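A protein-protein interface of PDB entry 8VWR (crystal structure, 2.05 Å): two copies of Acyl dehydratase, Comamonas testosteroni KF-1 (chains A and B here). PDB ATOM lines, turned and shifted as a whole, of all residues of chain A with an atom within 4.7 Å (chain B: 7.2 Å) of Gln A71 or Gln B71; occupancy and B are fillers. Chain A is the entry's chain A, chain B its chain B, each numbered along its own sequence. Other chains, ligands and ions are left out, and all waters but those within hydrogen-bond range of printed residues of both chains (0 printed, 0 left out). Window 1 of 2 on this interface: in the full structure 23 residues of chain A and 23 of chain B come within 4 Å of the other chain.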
ATOM      1  N   GLY A  67      17.484  26.960 -23.927  1.00  0.00           N
ATOM      2  CA  GLY A  67      16.162  26.383 -23.740  1.00  0.00           C
ATOM      3  C   GLY A  67      16.218  24.927 -23.318  1.00  0.00           C
ATOM      4  O   GLY A  67      15.502  24.509 -22.402  1.00  0.00           O
ATOM      5  N   ALA A  68      17.071  24.137 -23.971  1.00  0.00           N
ATOM      6  CA  ALA A  68      17.151  22.718 -23.646  1.00  0.00           C
ATOM      7  C   ALA A  68      17.792  22.488 -22.283  1.00  0.00           C
ATOM      8  O   ALA A  68      17.542  21.457 -21.649  1.00  0.00           O
ATOM      9  CB  ALA A  68      17.928  21.968 -24.728  1.00  0.00           C
ATOM     10  N   LEU A  69      18.622  23.426 -21.818  1.00  0.00           N
ATOM     11  CA  LEU A  69      19.170  23.319 -20.471  1.00  0.00           C
ATOM     12  C   LEU A  69      18.071  23.453 -19.422  1.00  0.00           C
ATOM     13  O   LEU A  69      17.999  22.657 -18.479  1.00  0.00           O
ATOM     14  CB  LEU A  69      20.242  24.386 -20.247  1.00  0.00           C
ATOM     15  CG  LEU A  69      20.647  24.601 -18.785  1.00  0.00           C
ATOM     16  CD1 LEU A  69      21.132  23.301 -18.159  1.00  0.00           C
ATOM     17  CD2 LEU A  69      21.710  25.693 -18.669  1.00  0.00           C
ATOM     18  N   VAL A  70      17.227  24.477 -19.553  1.00  0.00           N
ATOM     19  CA  VAL A  70      16.115  24.633 -18.619  1.00  0.00           C
ATOM     20  C   VAL A  70      15.226  23.394 -18.657  1.00  0.00           C
ATOM     21  O   VAL A  70      14.785  22.895 -17.614  1.00  0.00           O
ATOM     22  CB  VAL A  70      15.329  25.919 -18.938  1.00  0.00           C
ATOM     23  CG1 VAL A  70      14.150  26.076 -17.996  1.00  0.00           C
ATOM     24  CG2 VAL A  70      16.235  27.145 -18.841  1.00  0.00           C
ATOM     25  N   GLN A  71      14.980  22.860 -19.858  1.00  0.00           N
ATOM     26  CA  GLN A  71      14.170  21.652 -19.994  1.00  0.00           C
ATOM     27  C   GLN A  71      14.711  20.513 -19.137  1.00  0.00           C
ATOM     28  O   GLN A  71      13.964  19.875 -18.387  1.00  0.00           O
ATOM     29  CB  GLN A  71      14.113  21.230 -21.468  1.00  0.00           C
ATOM     30  CG  GLN A  71      13.460  19.871 -21.731  1.00  0.00           C
ATOM     31  CD  GLN A  71      13.959  19.215 -23.015  1.00  0.00           C
ATOM     32  OE1 GLN A  71      14.380  19.895 -23.950  1.00  0.00           O
ATOM     33  NE2 GLN A  71      13.926  17.889 -23.057  1.00  0.00           N
ATOM     34  N   VAL A  72      16.010  20.221 -19.253  1.00  0.00           N
ATOM     35  CA  VAL A  72      16.539  19.052 -18.555  1.00  0.00           C
ATOM     36  C   VAL A  72      16.743  19.310 -17.066  1.00  0.00           C
ATOM     37  O   VAL A  72      16.770  18.354 -16.283  1.00  0.00           O
ATOM     38  CB  VAL A  72      17.853  18.567 -19.193  1.00  0.00           C
ATOM     39  CG1 VAL A  72      17.639  18.259 -20.675  1.00  0.00           C
ATOM     40  CG2 VAL A  72      18.964  19.585 -19.001  1.00  0.00           C
ATOM     41  N   LEU A  73      16.879  20.573 -16.648  1.00  0.00           N
ATOM     42  CA  LEU A  73      16.945  20.895 -15.226  1.00  0.00           C
ATOM     43  C   LEU A  73      15.629  20.645 -14.500  1.00  0.00           C
ATOM     44  O   LEU A  73      15.551  20.889 -13.292  1.00  0.00           O
ATOM     45  CB  LEU A  73      17.358  22.356 -15.026  1.00  0.00           C
ATOM     46  CG  LEU A  73      18.808  22.700 -15.370  1.00  0.00           C
ATOM     47  CD1 LEU A  73      19.068  24.186 -15.173  1.00  0.00           C
ATOM     48  CD2 LEU A  73      19.786  21.878 -14.540  1.00  0.00           C
ATOM     49  N   ALA A  74      14.593  20.179 -15.201  1.00  0.00           N
ATOM     50  CA  ALA A  74      13.365  19.789 -14.519  1.00  0.00           C
ATOM     51  C   ALA A  74      13.619  18.681 -13.506  1.00  0.00           C
ATOM     52  O   ALA A  74      12.882  18.561 -12.520  1.00  0.00           O
ATOM     53  CB  ALA A  74      12.321  19.338 -15.541  1.00  0.00           C
ATOM     54  N   LEU A  99       7.235  21.061 -27.111  1.00  0.00           N
ATOM     55  CA  LEU A  99       8.325  21.742 -26.422  1.00  0.00           C
ATOM     56  C   LEU A  99       8.355  23.175 -26.928  1.00  0.00           C
ATOM     57  O   LEU A  99       8.453  23.405 -28.138  1.00  0.00           O
ATOM     58  CB  LEU A  99       9.652  21.032 -26.680  1.00  0.00           C
ATOM     59  CG  LEU A  99      10.754  21.196 -25.635  1.00  0.00           C
ATOM     60  CD1 LEU A  99      10.289  20.737 -24.260  1.00  0.00           C
ATOM     61  CD2 LEU A  99      11.988  20.418 -26.083  1.00  0.00           C
ATOM     62  N   ILE A 135       7.885  25.335 -16.611  1.00  0.00           N
ATOM     63  CA  ILE A 135       9.049  25.794 -15.860  1.00  0.00           C
ATOM     64  C   ILE A 135       9.099  27.314 -15.981  1.00  0.00           C
ATOM     65  O   ILE A 135       9.128  27.851 -17.095  1.00  0.00           O
ATOM     66  CB  ILE A 135      10.345  25.161 -16.377  1.00  0.00           C
ATOM     67  CG1 ILE A 135      10.210  23.638 -16.452  1.00  0.00           C
ATOM     68  CG2 ILE A 135      11.519  25.540 -15.484  1.00  0.00           C
ATOM     69  CD1 ILE A 135      11.426  22.950 -17.040  1.00  0.00           C
ATOM     70  N   VAL A 145       9.690  27.545 -20.175  1.00  0.00           N
ATOM     71  CA  VAL A 145       9.729  26.282 -20.905  1.00  0.00           C
ATOM     72  C   VAL A 145       8.409  25.555 -20.689  1.00  0.00           C
ATOM     73  O   VAL A 145       7.980  25.360 -19.547  1.00  0.00           O
ATOM     74  CB  VAL A 145      10.903  25.388 -20.459  1.00  0.00           C
ATOM     75  CG1 VAL A 145      10.741  23.976 -21.020  1.00  0.00           C
ATOM     76  CG2 VAL A 145      12.225  25.991 -20.896  1.00  0.00           C
ATOM     77  N   ASN A 147       6.571  21.883 -21.641  1.00  0.00           N
ATOM     78  CA  ASN A 147       6.945  20.526 -22.028  1.00  0.00           C
ATOM     79  C   ASN A 147       5.759  19.608 -21.767  1.00  0.00           C
ATOM     80  O   ASN A 147       5.445  19.308 -20.611  1.00  0.00           O
ATOM     81  CB  ASN A 147       8.183  20.056 -21.261  1.00  0.00           C
ATOM     82  CG  ASN A 147       8.693  18.707 -21.740  1.00  0.00           C
ATOM     83  OD1 ASN A 147       8.110  18.091 -22.631  1.00  0.00           O
ATOM     84  ND2 ASN A 147       9.795  18.248 -21.152  1.00  0.00           N
ATOM     85  N   SER B  41      21.731  17.555 -14.537  1.00  0.00           N
ATOM     86  CA  SER B  41      20.277  17.582 -14.609  1.00  0.00           C
ATOM     87  C   SER B  41      19.604  17.159 -13.311  1.00  0.00           C
ATOM     88  O   SER B  41      18.451  17.538 -13.077  1.00  0.00           O
ATOM     89  CB  SER B  41      19.792  16.667 -15.736  1.00  0.00           C
ATOM     90  OG  SER B  41      19.981  15.304 -15.392  1.00  0.00           O
ATOM     91  N   HIS B  66      20.658   8.843 -20.865  1.00  0.00           N
ATOM     92  CA  HIS B  66      19.368   9.512 -20.779  1.00  0.00           C
ATOM     93  C   HIS B  66      18.902   9.898 -22.178  1.00  0.00           C
ATOM     94  O   HIS B  66      19.692  10.368 -23.002  1.00  0.00           O
ATOM     95  CB  HIS B  66      19.448  10.780 -19.924  1.00  0.00           C
ATOM     96  CG  HIS B  66      20.156  10.610 -18.617  1.00  0.00           C
ATOM     97  ND1 HIS B  66      21.502  10.331 -18.528  1.00  0.00           N
ATOM     98  CD2 HIS B  66      19.713  10.732 -17.343  1.00  0.00           C
ATOM     99  CE1 HIS B  66      21.852  10.258 -17.255  1.00  0.00           C
ATOM    100  NE2 HIS B  66      20.785  10.504 -16.516  1.00  0.00           N
ATOM    101  N   GLY B  67      17.608   9.723 -22.442  1.00  0.00           N
ATOM    102  CA  GLY B  67      17.076  10.151 -23.725  1.00  0.00           C
ATOM    103  C   GLY B  67      17.345  11.618 -24.000  1.00  0.00           C
ATOM    104  O   GLY B  67      17.734  11.992 -25.110  1.00  0.00           O
ATOM    105  N   ALA B  68      17.153  12.469 -22.988  1.00  0.00           N
ATOM    106  CA  ALA B  68      17.364  13.900 -23.157  1.00  0.00           C
ATOM    107  C   ALA B  68      18.840  14.256 -23.272  1.00  0.00           C
ATOM    108  O   ALA B  68      19.170  15.305 -23.836  1.00  0.00           O
ATOM    109  CB  ALA B  68      16.734  14.664 -21.989  1.00  0.00           C
ATOM    110  N   LEU B  69      19.730  13.417 -22.741  1.00  0.00           N
ATOM    111  CA  LEU B  69      21.153  13.602 -22.990  1.00  0.00           C
ATOM    112  C   LEU B  69      21.468  13.430 -24.472  1.00  0.00           C
ATOM    113  O   LEU B  69      22.120  14.284 -25.084  1.00  0.00           O
ATOM    114  CB  LEU B  69      21.969  12.613 -22.159  1.00  0.00           C
ATOM    115  CG  LEU B  69      23.452  12.509 -22.525  1.00  0.00           C
ATOM    116  CD1 LEU B  69      24.105  13.880 -22.467  1.00  0.00           C
ATOM    117  CD2 LEU B  69      24.176  11.526 -21.609  1.00  0.00           C
ATOM    118  N   VAL B  70      21.026  12.318 -25.062  1.00  0.00           N
ATOM    119  CA  VAL B  70      21.244  12.113 -26.492  1.00  0.00           C
ATOM    120  C   VAL B  70      20.628  13.263 -27.279  1.00  0.00           C
ATOM    121  O   VAL B  70      21.191  13.723 -28.279  1.00  0.00           O
ATOM    122  CB  VAL B  70      20.682  10.747 -26.931  1.00  0.00           C
ATOM    123  CG1 VAL B  70      20.901  10.516 -28.430  1.00  0.00           C
ATOM    124  CG2 VAL B  70      21.329   9.619 -26.129  1.00  0.00           C
ATOM    125  N   GLN B  71      19.480  13.769 -26.815  1.00  0.00           N
ATOM    126  CA  GLN B  71      18.823  14.893 -27.475  1.00  0.00           C
ATOM    127  C   GLN B  71      19.738  16.112 -27.539  1.00  0.00           C
ATOM    128  O   GLN B  71      19.969  16.675 -28.614  1.00  0.00           O
ATOM    129  CB  GLN B  71      17.521  15.239 -26.740  1.00  0.00           C
ATOM    130  CG  GLN B  71      16.845  16.535 -27.201  1.00  0.00           C
ATOM    131  CD  GLN B  71      15.904  17.118 -26.154  1.00  0.00           C
ATOM    132  OE1 GLN B  71      15.420  16.408 -25.270  1.00  0.00           O
ATOM    133  NE2 GLN B  71      15.650  18.418 -26.246  1.00  0.00           N
ATOM    134  N   VAL B  72      20.251  16.557 -26.388  1.00  0.00           N
ATOM    135  CA  VAL B  72      21.032  17.789 -26.388  1.00  0.00           C
ATOM    136  C   VAL B  72      22.399  17.588 -27.036  1.00  0.00           C
ATOM    137  O   VAL B  72      23.014  18.564 -27.480  1.00  0.00           O
ATOM    138  CB  VAL B  72      21.185  18.357 -24.963  1.00  0.00           C
ATOM    139  CG1 VAL B  72      19.814  18.558 -24.324  1.00  0.00           C
ATOM    140  CG2 VAL B  72      22.060  17.462 -24.107  1.00  0.00           C
ATOM    141  N   LEU B  73      22.888  16.348 -27.119  1.00  0.00           N
ATOM    142  CA  LEU B  73      24.147  16.081 -27.808  1.00  0.00           C
ATOM    143  C   LEU B  73      24.044  16.280 -29.318  1.00  0.00           C
ATOM    144  O   LEU B  73      25.060  16.154 -30.011  1.00  0.00           O
ATOM    145  CB  LEU B  73      24.625  14.660 -27.497  1.00  0.00           C
ATOM    146  CG  LEU B  73      25.126  14.405 -26.071  1.00  0.00           C
ATOM    147  CD1 LEU B  73      25.467  12.926 -25.876  1.00  0.00           C
ATOM    148  CD2 LEU B  73      26.333  15.284 -25.742  1.00  0.00           C
ATOM    149  N   ALA B  74      22.859  16.591 -29.845  1.00  0.00           N
ATOM    150  CA  ALA B  74      22.750  16.938 -31.257  1.00  0.00           C
ATOM    151  C   ALA B  74      23.678  18.092 -31.619  1.00  0.00           C
ATOM    152  O   ALA B  74      24.153  18.174 -32.757  1.00  0.00           O
ATOM    153  CB  ALA B  74      21.303  17.289 -31.599  1.00  0.00           C
ATOM    154  N   SER B  75      23.959  18.985 -30.668  1.00  0.00           N
ATOM    155  CA  SER B  75      24.849  20.108 -30.940  1.00  0.00           C
ATOM    156  C   SER B  75      26.311  19.695 -31.050  1.00  0.00           C
ATOM    157  O   SER B  75      27.156  20.555 -31.316  1.00  0.00           O
ATOM    158  CB  SER B  75      24.675  21.172 -29.859  1.00  0.00           C
ATOM    159  OG  SER B  75      23.363  21.707 -29.912  1.00  0.00           O
ATOM    160  N   SER B  96       9.928  22.095 -30.279  1.00  0.00           N
ATOM    161  CA  SER B  96       9.724  20.818 -30.947  1.00  0.00           C
ATOM    162  C   SER B  96       8.246  20.463 -30.922  1.00  0.00           C
ATOM    163  O   SER B  96       7.519  20.822 -29.991  1.00  0.00           O
ATOM    164  CB  SER B  96      10.549  19.704 -30.287  1.00  0.00           C
ATOM    165  OG  SER B  96      10.255  18.438 -30.853  1.00  0.00           O
ATOM    166  N   LEU B  99       9.016  14.586 -29.659  1.00  0.00           N
ATOM    167  CA  LEU B  99      10.257  14.040 -29.135  1.00  0.00           C
ATOM    168  C   LEU B  99       9.993  12.604 -28.705  1.00  0.00           C
ATOM    169  O   LEU B  99       9.067  12.351 -27.929  1.00  0.00           O
ATOM    170  CB  LEU B  99      10.769  14.881 -27.962  1.00  0.00           C
ATOM    171  CG  LEU B  99      12.122  14.494 -27.367  1.00  0.00           C
ATOM    172  CD1 LEU B  99      13.256  14.704 -28.364  1.00  0.00           C
ATOM    173  CD2 LEU B  99      12.369  15.290 -26.093  1.00  0.00           C
ATOM    174  N   PHE B 101      12.046   8.572 -27.861  1.00  0.00           N
ATOM    175  CA  PHE B 101      13.267   7.823 -27.556  1.00  0.00           C
ATOM    176  C   PHE B 101      13.021   6.354 -27.891  1.00  0.00           C
ATOM    177  O   PHE B 101      12.807   5.528 -26.994  1.00  0.00           O
ATOM    178  CB  PHE B 101      13.673   7.977 -26.087  1.00  0.00           C
ATOM    179  CG  PHE B 101      13.623   9.392 -25.583  1.00  0.00           C
ATOM    180  CD1 PHE B 101      14.402  10.379 -26.161  1.00  0.00           C
ATOM    181  CD2 PHE B 101      12.811   9.729 -24.512  1.00  0.00           C
ATOM    182  CE1 PHE B 101      14.359  11.679 -25.694  1.00  0.00           C
ATOM    183  CE2 PHE B 101      12.764  11.027 -24.040  1.00  0.00           C
ATOM    184  CZ  PHE B 101      13.539  12.002 -24.630  1.00  0.00           C
ATOM    185  N   ILE B 111      27.285   7.880 -31.535  1.00  0.00           N
ATOM    186  CA  ILE B 111      26.039   8.294 -32.162  1.00  0.00           C
ATOM    187  C   ILE B 111      26.355   9.157 -33.377  1.00  0.00           C
ATOM    188  O   ILE B 111      27.463   9.677 -33.539  1.00  0.00           O
ATOM    189  CB  ILE B 111      25.110   9.053 -31.187  1.00  0.00           C
ATOM    190  CG1 ILE B 111      25.847  10.228 -30.540  1.00  0.00           C
ATOM    191  CG2 ILE B 111      24.561   8.095 -30.134  1.00  0.00           C
ATOM    192  CD1 ILE B 111      24.966  11.122 -29.674  1.00  0.00           C
ATOM    193  N   LEU B 133      14.766  15.551 -36.971  1.00  0.00           N
ATOM    194  CA  LEU B 133      16.127  15.161 -36.623  1.00  0.00           C
ATOM    195  C   LEU B 133      16.101  13.741 -36.069  1.00  0.00           C
ATOM    196  O   LEU B 133      15.306  13.437 -35.175  1.00  0.00           O
ATOM    197  CB  LEU B 133      16.711  16.133 -35.597  1.00  0.00           C
ATOM    198  CG  LEU B 133      18.095  15.825 -35.028  1.00  0.00           C
ATOM    199  CD1 LEU B 133      19.131  15.735 -36.127  1.00  0.00           C
ATOM    200  CD2 LEU B 133      18.481  16.892 -34.008  1.00  0.00           C
ATOM    201  N   ILE B 135      18.642  10.855 -34.437  1.00  0.00           N
ATOM    202  CA  ILE B 135      19.933  10.521 -33.841  1.00  0.00           C
ATOM    203  C   ILE B 135      19.976   9.015 -33.613  1.00  0.00           C
ATOM    204  O   ILE B 135      19.079   8.453 -32.969  1.00  0.00           O
ATOM    205  CB  ILE B 135      20.163  11.284 -32.526  1.00  0.00           C
ATOM    206  CG1 ILE B 135      19.961  12.789 -32.733  1.00  0.00           C
ATOM    207  CG2 ILE B 135      21.565  11.009 -31.997  1.00  0.00           C
ATOM    208  CD1 ILE B 135      19.962  13.598 -31.451  1.00  0.00           C
ATOM    209  N   VAL B 145      16.802   8.828 -30.951  1.00  0.00           N
ATOM    210  CA  VAL B 145      16.031  10.028 -30.643  1.00  0.00           C
ATOM    211  C   VAL B 145      15.392  10.540 -31.928  1.00  0.00           C
ATOM    212  O   VAL B 145      16.064  10.656 -32.959  1.00  0.00           O
ATOM    213  CB  VAL B 145      16.893  11.143 -30.016  1.00  0.00           C
ATOM    214  CG1 VAL B 145      16.061  12.417 -29.842  1.00  0.00           C
ATOM    215  CG2 VAL B 145      17.471  10.695 -28.689  1.00  0.00           C
ATOM    216  N   ILE B 146      14.099  10.843 -31.864  1.00  0.00           N
ATOM    217  CA  ILE B 146      13.386  11.554 -32.919  1.00  0.00           C
ATOM    218  C   ILE B 146      12.990  12.910 -32.351  1.00  0.00           C
ATOM    219  O   ILE B 146      12.403  12.984 -31.264  1.00  0.00           O
ATOM    220  CB  ILE B 146      12.153  10.768 -33.400  1.00  0.00           C
ATOM    221  CG1 ILE B 146      12.576   9.392 -33.926  1.00  0.00           C
ATOM    222  CG2 ILE B 146      11.410  11.545 -34.486  1.00  0.00           C
ATOM    223  CD1 ILE B 146      11.424   8.493 -34.304  1.00  0.00           C
ATOM    224  N   ASN B 147      13.331  13.983 -33.065  1.00  0.00           N
ATOM    225  CA  ASN B 147      13.051  15.343 -32.607  1.00  0.00           C
ATOM    226  C   ASN B 147      12.598  16.168 -33.804  1.00  0.00           C
ATOM    227  O   ASN B 147      13.403  16.475 -34.688  1.00  0.00           O
ATOM    228  CB  ASN B 147      14.285  15.964 -31.941  1.00  0.00           C
ATOM    229  CG  ASN B 147      13.985  17.292 -31.253  1.00  0.00           C
ATOM    230  OD1 ASN B 147      12.856  17.785 -31.283  1.00  0.00           O
ATOM    231  ND2 ASN B 147      15.002  17.871 -30.616  1.00  0.00           N
ATOM    232  N   LEU B 149      12.117  19.347 -34.911  1.00  0.00           N
ATOM    233  CA  LEU B 149      12.475  20.716 -34.567  1.00  0.00           C
ATOM    234  C   LEU B 149      11.602  21.720 -35.310  1.00  0.00           C
ATOM    235  O   LEU B 149      11.344  21.573 -36.506  1.00  0.00           O
ATOM    236  CB  LEU B 149      13.940  20.974 -34.911  1.00  0.00           C
ATOM    237  CG  LEU B 149      14.969  20.151 -34.142  1.00  0.00           C
ATOM    238  CD1 LEU B 149      16.336  20.243 -34.803  1.00  0.00           C
ATOM    239  CD2 LEU B 149      15.029  20.622 -32.697  1.00  0.00           C
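The side-chain amide oxygen (OE1) of Gln A71 lies within hydrogen-bond range of the side-chain amide nitrogen (NE2) of Gln B71.
The backbone carbonyl oxygen (O) of Ser B96 is in hydrogen-bond range of the backbone NH (N) of Leu A99, at 2.9 Å.
OG of Ser B96 sits at hydrogen-bond distance from OD1 of Asn B147 (2.7 Å).
Of the 12 printed residues of chain A, 4 touch a printed residue of chain B.
Hydrophobic or aromatic side chains of chain A that line the printed part of chain B: Ala A68, Val A72 and Leu A99.
Among the printed residues, 5 pairs touch across the chains.
Among the printed residues, no Asp or Glu carboxylate lies within 4 Å of a Lys or Arg side-chain nitrogen of the other chain.
Ala A68 touches Val B72 (CB to CG1, 3.9 Å).
Val A72 touches Ser B41.
Ala B68 touches Val A72.
Ala A68 touches Val B72, and with the chains exchanged Val A72 touches Ala B68.
Gln A71 touches its own counterpart, Gln B71.
Of the 5 pairs that touch across the chains among the printed residues, 3 have their exchanged pair printed and touching as well.
Printed residues of chain A within 4 Å of Gln B71: Gln A71 (3.0 Å).
Printed residues of chain A within 4 Å of Val B72: Ala A68.
Of the printed residues of chain B, Ala A68 touches Val B72.
Printed residues of chain A within 4 Å of Ser B41: Val A72.
Leu B73 touches none of the printed residues of chain A.
The nearest residue of chain B that does not touch Gln A71 is Leu B99 (4.3 Å).
The nearest residue of chain A that does not touch Gln B71 is Leu A99 (4.2 Å).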
